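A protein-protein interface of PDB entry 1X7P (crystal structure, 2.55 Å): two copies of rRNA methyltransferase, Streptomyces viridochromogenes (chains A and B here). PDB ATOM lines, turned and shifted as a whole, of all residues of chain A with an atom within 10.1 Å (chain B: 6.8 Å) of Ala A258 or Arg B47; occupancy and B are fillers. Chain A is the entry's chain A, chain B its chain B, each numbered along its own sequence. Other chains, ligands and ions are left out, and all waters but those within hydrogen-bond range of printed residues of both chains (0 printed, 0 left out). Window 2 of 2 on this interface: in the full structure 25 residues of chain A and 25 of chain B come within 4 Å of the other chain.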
ATOM      1  N   GLU A 212      10.427 -36.790  -0.529  1.00  0.00           N
ATOM      2  CA  GLU A 212       9.887 -35.544  -1.087  1.00  0.00           C
ATOM      3  C   GLU A 212       9.261 -35.702  -2.476  1.00  0.00           C
ATOM      4  O   GLU A 212       8.341 -34.984  -2.824  1.00  0.00           O
ATOM      5  CB  GLU A 212      10.985 -34.480  -1.158  1.00  0.00           C
ATOM      6  CG  GLU A 212      12.145 -34.862  -2.056  1.00  0.00           C
ATOM      7  CD  GLU A 212      13.262 -33.851  -2.027  1.00  0.00           C
ATOM      8  OE1 GLU A 212      14.163 -33.976  -1.151  1.00  0.00           O
ATOM      9  OE2 GLU A 212      13.234 -32.948  -2.897  1.00  0.00           O
ATOM     10  N   HIS A 213       9.794 -36.636  -3.251  1.00  0.00           N
ATOM     11  CA  HIS A 213       9.357 -36.916  -4.617  1.00  0.00           C
ATOM     12  C   HIS A 213       8.614 -38.245  -4.669  1.00  0.00           C
ATOM     13  O   HIS A 213       8.740 -38.982  -5.631  1.00  0.00           O
ATOM     14  CB  HIS A 213      10.576 -37.008  -5.538  1.00  0.00           C
ATOM     15  CG  HIS A 213      11.180 -35.688  -5.896  1.00  0.00           C
ATOM     16  ND1 HIS A 213      10.914 -34.529  -5.201  1.00  0.00           N
ATOM     17  CD2 HIS A 213      12.022 -35.340  -6.898  1.00  0.00           C
ATOM     18  CE1 HIS A 213      11.577 -33.526  -5.746  1.00  0.00           C
ATOM     19  NE2 HIS A 213      12.248 -33.988  -6.786  1.00  0.00           N
ATOM     20  N   MET A 254       5.792 -29.795  -0.829  1.00  0.00           N
ATOM     21  CA  MET A 254       6.645 -28.680  -0.434  1.00  0.00           C
ATOM     22  C   MET A 254       6.340 -27.422  -1.248  1.00  0.00           C
ATOM     23  O   MET A 254       5.685 -27.484  -2.284  1.00  0.00           O
ATOM     24  CB  MET A 254       8.148 -29.020  -0.565  1.00  0.00           C
ATOM     25  CG  MET A 254       8.594 -30.431  -0.146  1.00  0.00           C
ATOM     26  SD  MET A 254       9.479 -30.523   1.431  1.00  0.00           S
ATOM     27  CE  MET A 254       8.118 -30.121   2.513  1.00  0.00           C
ATOM     28  N   ALA A 255       6.875 -26.294  -0.785  1.00  0.00           N
ATOM     29  CA  ALA A 255       6.600 -24.974  -1.350  1.00  0.00           C
ATOM     30  C   ALA A 255       7.330 -24.748  -2.664  1.00  0.00           C
ATOM     31  O   ALA A 255       6.813 -24.080  -3.579  1.00  0.00           O
ATOM     32  CB  ALA A 255       7.001 -23.897  -0.366  1.00  0.00           C
ATOM     33  N   GLY A 256       8.551 -25.270  -2.755  1.00  0.00           N
ATOM     34  CA  GLY A 256       9.296 -25.205  -4.006  1.00  0.00           C
ATOM     35  C   GLY A 256      10.191 -26.406  -4.223  1.00  0.00           C
ATOM     36  O   GLY A 256      10.103 -27.420  -3.512  1.00  0.00           O
ATOM     37  N   SER A 257      11.063 -26.283  -5.217  1.00  0.00           N
ATOM     38  CA  SER A 257      12.153 -27.247  -5.412  1.00  0.00           C
ATOM     39  C   SER A 257      13.377 -26.878  -4.532  1.00  0.00           C
ATOM     40  O   SER A 257      14.417 -27.545  -4.595  1.00  0.00           O
ATOM     41  CB  SER A 257      12.541 -27.330  -6.902  1.00  0.00           C
ATOM     42  OG  SER A 257      11.993 -26.262  -7.651  1.00  0.00           O
ATOM     43  N   ALA A 258      13.244 -25.820  -3.721  1.00  0.00           N
ATOM     44  CA  ALA A 258      14.315 -25.364  -2.825  1.00  0.00           C
ATOM     45  C   ALA A 258      14.346 -26.171  -1.522  1.00  0.00           C
ATOM     46  O   ALA A 258      14.940 -27.270  -1.488  1.00  0.00           O
ATOM     47  CB  ALA A 258      14.187 -23.843  -2.541  1.00  0.00           C
ATOM     48  N   SER A 259      13.700 -25.682  -0.460  1.00  0.00           N
ATOM     49  CA  SER A 259      13.847 -26.343   0.827  1.00  0.00           C
ATOM     50  C   SER A 259      13.452 -27.819   0.742  1.00  0.00           C
ATOM     51  O   SER A 259      12.894 -28.246  -0.264  1.00  0.00           O
ATOM     52  CB  SER A 259      13.068 -25.619   1.939  1.00  0.00           C
ATOM     53  OG  SER A 259      13.511 -26.036   3.250  1.00  0.00           O
ATOM     54  N   SER A 260      13.851 -28.576   1.778  1.00  0.00           N
ATOM     55  CA  SER A 260      13.393 -29.951   2.097  1.00  0.00           C
ATOM     56  C   SER A 260      13.254 -30.033   3.635  1.00  0.00           C
ATOM     57  O   SER A 260      13.506 -29.034   4.298  1.00  0.00           O
ATOM     58  CB  SER A 260      14.396 -30.991   1.605  1.00  0.00           C
ATOM     59  OG  SER A 260      14.077 -32.301   2.076  1.00  0.00           O
ATOM     60  N   LEU A 261      12.835 -31.172   4.212  1.00  0.00           N
ATOM     61  CA  LEU A 261      12.643 -31.262   5.677  1.00  0.00           C
ATOM     62  C   LEU A 261      13.686 -32.142   6.393  1.00  0.00           C
ATOM     63  O   LEU A 261      14.134 -33.142   5.850  1.00  0.00           O
ATOM     64  CB  LEU A 261      11.233 -31.762   6.025  1.00  0.00           C
ATOM     65  CG  LEU A 261       9.979 -30.971   5.602  1.00  0.00           C
ATOM     66  CD1 LEU A 261       8.698 -31.751   5.955  1.00  0.00           C
ATOM     67  CD2 LEU A 261       9.921 -29.605   6.245  1.00  0.00           C
ATOM     68  N   MET B  44      28.508 -21.182   6.209  1.00  0.00           N
ATOM     69  CA  MET B  44      29.385 -22.136   5.530  1.00  0.00           C
ATOM     70  C   MET B  44      28.628 -23.038   4.567  1.00  0.00           C
ATOM     71  O   MET B  44      27.462 -23.372   4.796  1.00  0.00           O
ATOM     72  CB  MET B  44      30.192 -22.986   6.526  1.00  0.00           C
ATOM     73  CG  MET B  44      29.417 -23.573   7.702  1.00  0.00           C
ATOM     74  SD  MET B  44      30.127 -23.059   9.301  1.00  0.00           S
ATOM     75  CE  MET B  44      31.139 -24.561   9.784  1.00  0.00           C
ATOM     76  N   GLY B  45      29.310 -23.411   3.480  1.00  0.00           N
ATOM     77  CA  GLY B  45      28.787 -24.320   2.481  1.00  0.00           C
ATOM     78  C   GLY B  45      28.478 -23.601   1.184  1.00  0.00           C
ATOM     79  O   GLY B  45      27.855 -22.537   1.181  1.00  0.00           O
ATOM     80  N   VAL B  46      28.888 -24.187   0.067  1.00  0.00           N
ATOM     81  CA  VAL B  46      28.564 -23.595  -1.222  1.00  0.00           C
ATOM     82  C   VAL B  46      27.042 -23.354  -1.354  1.00  0.00           C
ATOM     83  O   VAL B  46      26.625 -22.289  -1.811  1.00  0.00           O
ATOM     84  CB  VAL B  46      29.108 -24.427  -2.419  1.00  0.00           C
ATOM     85  CG1 VAL B  46      30.623 -24.478  -2.391  1.00  0.00           C
ATOM     86  CG2 VAL B  46      28.515 -25.845  -2.460  1.00  0.00           C
ATOM     87  N   ARG B  47      26.221 -24.310  -0.915  1.00  0.00           N
ATOM     88  CA  ARG B  47      24.771 -24.200  -1.101  1.00  0.00           C
ATOM     89  C   ARG B  47      24.167 -23.042  -0.297  1.00  0.00           C
ATOM     90  O   ARG B  47      23.492 -22.200  -0.886  1.00  0.00           O
ATOM     91  CB  ARG B  47      24.046 -25.526  -0.817  1.00  0.00           C
ATOM     92  CG  ARG B  47      22.659 -25.618  -1.441  1.00  0.00           C
ATOM     93  CD  ARG B  47      21.571 -26.223  -0.545  1.00  0.00           C
ATOM     94  NE  ARG B  47      20.483 -26.803  -1.345  1.00  0.00           N
ATOM     95  CZ  ARG B  47      19.179 -26.497  -1.236  1.00  0.00           C
ATOM     96  NH1 ARG B  47      18.717 -25.625  -0.336  1.00  0.00           N
ATOM     97  NH2 ARG B  47      18.316 -27.100  -2.042  1.00  0.00           N
ATOM     98  N   PRO B  48      24.385 -22.986   1.024  1.00  0.00           N
ATOM     99  CA  PRO B  48      23.943 -21.818   1.805  1.00  0.00           C
ATOM    100  C   PRO B  48      24.416 -20.463   1.250  1.00  0.00           C
ATOM    101  O   PRO B  48      23.571 -19.574   1.157  1.00  0.00           O
ATOM    102  CB  PRO B  48      24.528 -22.079   3.203  1.00  0.00           C
ATOM    103  CG  PRO B  48      24.646 -23.569   3.276  1.00  0.00           C
ATOM    104  CD  PRO B  48      24.986 -24.024   1.893  1.00  0.00           C
ATOM    105  N   ILE B  49      25.698 -20.309   0.887  1.00  0.00           N
ATOM    106  CA  ILE B  49      26.187 -19.027   0.355  1.00  0.00           C
ATOM    107  C   ILE B  49      25.435 -18.637  -0.929  1.00  0.00           C
ATOM    108  O   ILE B  49      25.134 -17.470  -1.153  1.00  0.00           O
ATOM    109  CB  ILE B  49      27.728 -19.026   0.021  1.00  0.00           C
ATOM    110  CG1 ILE B  49      28.625 -19.620   1.126  1.00  0.00           C
ATOM    111  CG2 ILE B  49      28.198 -17.601  -0.286  1.00  0.00           C
ATOM    112  CD1 ILE B  49      28.392 -19.098   2.484  1.00  0.00           C
ATOM    113  N   SER B  50      25.152 -19.611  -1.782  1.00  0.00           N
ATOM    114  CA  SER B  50      24.533 -19.307  -3.079  1.00  0.00           C
ATOM    115  C   SER B  50      23.113 -18.806  -2.885  1.00  0.00           C
ATOM    116  O   SER B  50      22.663 -17.916  -3.620  1.00  0.00           O
ATOM    117  CB  SER B  50      24.540 -20.518  -4.012  1.00  0.00           C
ATOM    118  OG  SER B  50      25.860 -21.013  -4.162  1.00  0.00           O
ATOM    119  N   LEU B  51      22.419 -19.379  -1.898  1.00  0.00           N
ATOM    120  CA  LEU B  51      21.080 -18.921  -1.535  1.00  0.00           C
ATOM    121  C   LEU B  51      21.127 -17.478  -1.017  1.00  0.00           C
ATOM    122  O   LEU B  51      20.251 -16.682  -1.338  1.00  0.00           O
ATOM    123  CB  LEU B  51      20.422 -19.864  -0.515  1.00  0.00           C
ATOM    124  CG  LEU B  51      20.011 -21.247  -1.030  1.00  0.00           C
ATOM    125  CD1 LEU B  51      19.582 -22.122   0.112  1.00  0.00           C
ATOM    126  CD2 LEU B  51      18.896 -21.161  -2.036  1.00  0.00           C
ATOM    127  N   ALA B  52      22.174 -17.144  -0.264  1.00  0.00           N
ATOM    128  CA  ALA B  52      22.369 -15.791   0.253  1.00  0.00           C
ATOM    129  C   ALA B  52      22.602 -14.779  -0.869  1.00  0.00           C
ATOM    130  O   ALA B  52      22.130 -13.646  -0.812  1.00  0.00           O
ATOM    131  CB  ALA B  52      23.541 -15.764   1.230  1.00  0.00           C
ATOM    132  N   HIS B  55      19.262 -14.311  -2.955  1.00  0.00           N
ATOM    133  CA  HIS B  55      18.166 -13.608  -2.293  1.00  0.00           C
ATOM    134  C   HIS B  55      18.590 -12.214  -1.812  1.00  0.00           C
ATOM    135  O   HIS B  55      17.988 -11.649  -0.893  1.00  0.00           O
ATOM    136  CB  HIS B  55      17.620 -14.458  -1.144  1.00  0.00           C
ATOM    137  CG  HIS B  55      16.768 -15.600  -1.596  1.00  0.00           C
ATOM    138  ND1 HIS B  55      15.403 -15.493  -1.741  1.00  0.00           N
ATOM    139  CD2 HIS B  55      17.088 -16.866  -1.954  1.00  0.00           C
ATOM    140  CE1 HIS B  55      14.915 -16.647  -2.168  1.00  0.00           C
ATOM    141  NE2 HIS B  55      15.918 -17.495  -2.311  1.00  0.00           N
ATOM    142  N   TRP B  73      31.113 -26.324  -7.980  1.00  0.00           N
ATOM    143  CA  TRP B  73      30.274 -25.299  -7.358  1.00  0.00           C
ATOM    144  C   TRP B  73      31.078 -24.194  -6.648  1.00  0.00           C
ATOM    145  O   TRP B  73      30.782 -23.014  -6.816  1.00  0.00           O
ATOM    146  CB  TRP B  73      29.332 -25.974  -6.352  1.00  0.00           C
ATOM    147  CG  TRP B  73      28.089 -25.203  -5.971  1.00  0.00           C
ATOM    148  CD1 TRP B  73      27.913 -23.842  -5.951  1.00  0.00           C
ATOM    149  CD2 TRP B  73      26.850 -25.768  -5.543  1.00  0.00           C
ATOM    150  NE1 TRP B  73      26.641 -23.535  -5.532  1.00  0.00           N
ATOM    151  CE2 TRP B  73      25.965 -24.697  -5.277  1.00  0.00           C
ATOM    152  CE3 TRP B  73      26.395 -27.081  -5.347  1.00  0.00           C
ATOM    153  CZ2 TRP B  73      24.662 -24.897  -4.833  1.00  0.00           C
ATOM    154  CZ3 TRP B  73      25.109 -27.280  -4.912  1.00  0.00           C
ATOM    155  CH2 TRP B  73      24.249 -26.189  -4.655  1.00  0.00           C
ATOM    156  N   LEU B  77      31.461 -20.228  -7.695  1.00  0.00           N
ATOM    157  CA  LEU B  77      31.170 -19.212  -6.688  1.00  0.00           C
ATOM    158  C   LEU B  77      32.194 -18.086  -6.740  1.00  0.00           C
ATOM    159  O   LEU B  77      31.842 -16.914  -6.679  1.00  0.00           O
ATOM    160  CB  LEU B  77      31.157 -19.814  -5.272  1.00  0.00           C
ATOM    161  CG  LEU B  77      29.836 -19.847  -4.498  1.00  0.00           C
ATOM    162  CD1 LEU B  77      30.133 -19.981  -3.006  1.00  0.00           C
ATOM    163  CD2 LEU B  77      28.951 -18.624  -4.757  1.00  0.00           C
ATOM    164  N   ASP B 148       9.849 -22.491   5.681  1.00  0.00           N
ATOM    165  CA  ASP B 148      10.258 -22.299   4.285  1.00  0.00           C
ATOM    166  C   ASP B 148       9.701 -23.422   3.424  1.00  0.00           C
ATOM    167  O   ASP B 148       9.074 -23.170   2.414  1.00  0.00           O
ATOM    168  CB  ASP B 148      11.790 -22.274   4.189  1.00  0.00           C
ATOM    169  CG  ASP B 148      12.303 -21.857   2.815  1.00  0.00           C
ATOM    170  OD1 ASP B 148      11.642 -21.064   2.130  1.00  0.00           O
ATOM    171  OD2 ASP B 148      13.395 -22.243   2.345  1.00  0.00           O
ATOM    172  N   ALA B 149       9.900 -24.669   3.854  1.00  0.00           N
ATOM    173  CA  ALA B 149       9.539 -25.826   3.043  1.00  0.00           C
ATOM    174  C   ALA B 149       8.026 -26.031   2.872  1.00  0.00           C
ATOM    175  O   ALA B 149       7.582 -26.549   1.853  1.00  0.00           O
ATOM    176  CB  ALA B 149      10.169 -27.051   3.608  1.00  0.00           C
ATOM    177  N   THR B 174      19.651 -24.795   7.044  1.00  0.00           N
ATOM    178  CA  THR B 174      20.067 -25.389   5.776  1.00  0.00           C
ATOM    179  C   THR B 174      19.917 -24.408   4.600  1.00  0.00           C
ATOM    180  O   THR B 174      19.628 -24.827   3.481  1.00  0.00           O
ATOM    181  CB  THR B 174      19.281 -26.728   5.534  1.00  0.00           C
ATOM    182  OG1 THR B 174      19.749 -27.730   6.453  1.00  0.00           O
ATOM    183  CG2 THR B 174      19.573 -27.360   4.160  1.00  0.00           C
ATOM    184  N   GLY B 175      20.107 -23.109   4.853  1.00  0.00           N
ATOM    185  CA  GLY B 175      19.959 -22.082   3.824  1.00  0.00           C
ATOM    186  C   GLY B 175      18.585 -21.429   3.675  1.00  0.00           C
ATOM    187  O   GLY B 175      18.428 -20.454   2.939  1.00  0.00           O
ATOM    188  N   SER B 176      17.585 -21.964   4.362  1.00  0.00           N
ATOM    189  CA  SER B 176      16.245 -21.378   4.390  1.00  0.00           C
ATOM    190  C   SER B 176      16.231 -20.008   5.035  1.00  0.00           C
ATOM    191  O   SER B 176      15.313 -19.241   4.832  1.00  0.00           O
ATOM    192  CB  SER B 176      15.325 -22.263   5.207  1.00  0.00           C
ATOM    193  OG  SER B 176      15.183 -23.492   4.562  1.00  0.00           O
ATOM    194  N   PHE B 178      17.812 -17.515   4.418  1.00  0.00           N
ATOM    195  CA  PHE B 178      17.890 -16.491   3.387  1.00  0.00           C
ATOM    196  C   PHE B 178      16.622 -16.326   2.542  1.00  0.00           C
ATOM    197  O   PHE B 178      16.375 -15.250   1.996  1.00  0.00           O
ATOM    198  CB  PHE B 178      19.091 -16.808   2.503  1.00  0.00           C
ATOM    199  CG  PHE B 178      20.358 -17.017   3.287  1.00  0.00           C
ATOM    200  CD1 PHE B 178      20.813 -16.038   4.158  1.00  0.00           C
ATOM    201  CD2 PHE B 178      21.062 -18.204   3.202  1.00  0.00           C
ATOM    202  CE1 PHE B 178      21.957 -16.228   4.898  1.00  0.00           C
ATOM    203  CE2 PHE B 178      22.214 -18.395   3.947  1.00  0.00           C
ATOM    204  CZ  PHE B 178      22.657 -17.408   4.791  1.00  0.00           C
ATOM    205  N   SER B 179      15.812 -17.376   2.437  1.00  0.00           N
ATOM    206  CA  SER B 179      14.557 -17.293   1.697  1.00  0.00           C
ATOM    207  C   SER B 179      13.338 -17.045   2.584  1.00  0.00           C
ATOM    208  O   SER B 179      12.302 -16.604   2.093  1.00  0.00           O
ATOM    209  CB  SER B 179      14.345 -18.549   0.849  1.00  0.00           C
ATOM    210  OG  SER B 179      14.140 -19.687   1.656  1.00  0.00           O
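The backbone NH (N) of Ala A255 lies within hydrogen-bond range of the backbone carbonyl oxygen (O) of Ala B149, at 2.7 Å.
The backbone carbonyl oxygen (O) of Ala A258 is in hydrogen-bond range of the guanidinium group (NH2) of Arg B47 (3.4 Å).
The side-chain hydroxyl of Ser A259 sits at hydrogen-bond distance from the side-chain hydroxyl of Ser B176 (3.3 Å).
OD2 of Asp B148 lies within hydrogen-bond range of OG of Ser B179, 2.8 Å away.
The backbone carbonyl oxygen (O) of Ser B176 is in hydrogen-bond range of the side-chain hydroxyl (OG) of Ser B179 (3.4 Å).
OD2 of Asp B148 lies within hydrogen-bond range of OG of Ser B176 (3.1 Å).
Met A254 touches Ala B149 (CA to O, 3.3 Å).
O of Asp B148 touches CB of Ala A255 (3.5 Å).
Ser A259 touches Asp B148 (CB to OD2, 3.4 Å).
Ser A259 touches Ala B149 (OG to CB, 3.5 Å).
Ala B149 touches Ser A260.
Leu A261 touches Ala B149 (CD2 to CB, 3.7 Å).
Printed residues of chain B within 4 Å of Met A254: Ala B149.
Ala A258 touches just one residue of chain B: Arg B47 (3.4 Å).
Of the printed residues of chain B, Ser A260 touches Ala B149.
Of the printed residues of chain B, Leu A261 touches Ala B149.
No residue of chain A comes within 4 Å of Gly B45.
Arg B47 touches one residue of chain A.
No residue of chain A comes within 4 Å of Ser B50.
Printed residues of chain A within 4 Å of Ala B149: Met A254 (3.3 Å), Ala A255 (2.7 Å), Ser A259 (3.5 Å), Ser A260 (3.9 Å) and Leu A261 (3.7 Å).
The nearest residue of chain B that does not touch Ala A258 is Asp B148 (5.2 Å).
The nearest residue of chain A that does not touch Arg B47 is Ser A257 (4.7 Å).
The nearest printed residue of chain B that does not touch Ser A259 is Arg B47 (5.0 Å).
Hydrophobic or aromatic side chains of chain A within 4 Å of the printed part of chain B: Met A254, Ala A255 and Leu A261.
Of the 19 printed residues of chain B, 4 touch a printed residue of chain A.
Hydrophobic or aromatic side chains of chain B that line the printed part of chain A: Ala B149.
Among the printed residues, 9 pairs touch across the chains.
No position is printed for both chains.
Of the 9 pairs that touch across the chains among the printed residues, none has its exchanged pair printed and touching as well.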
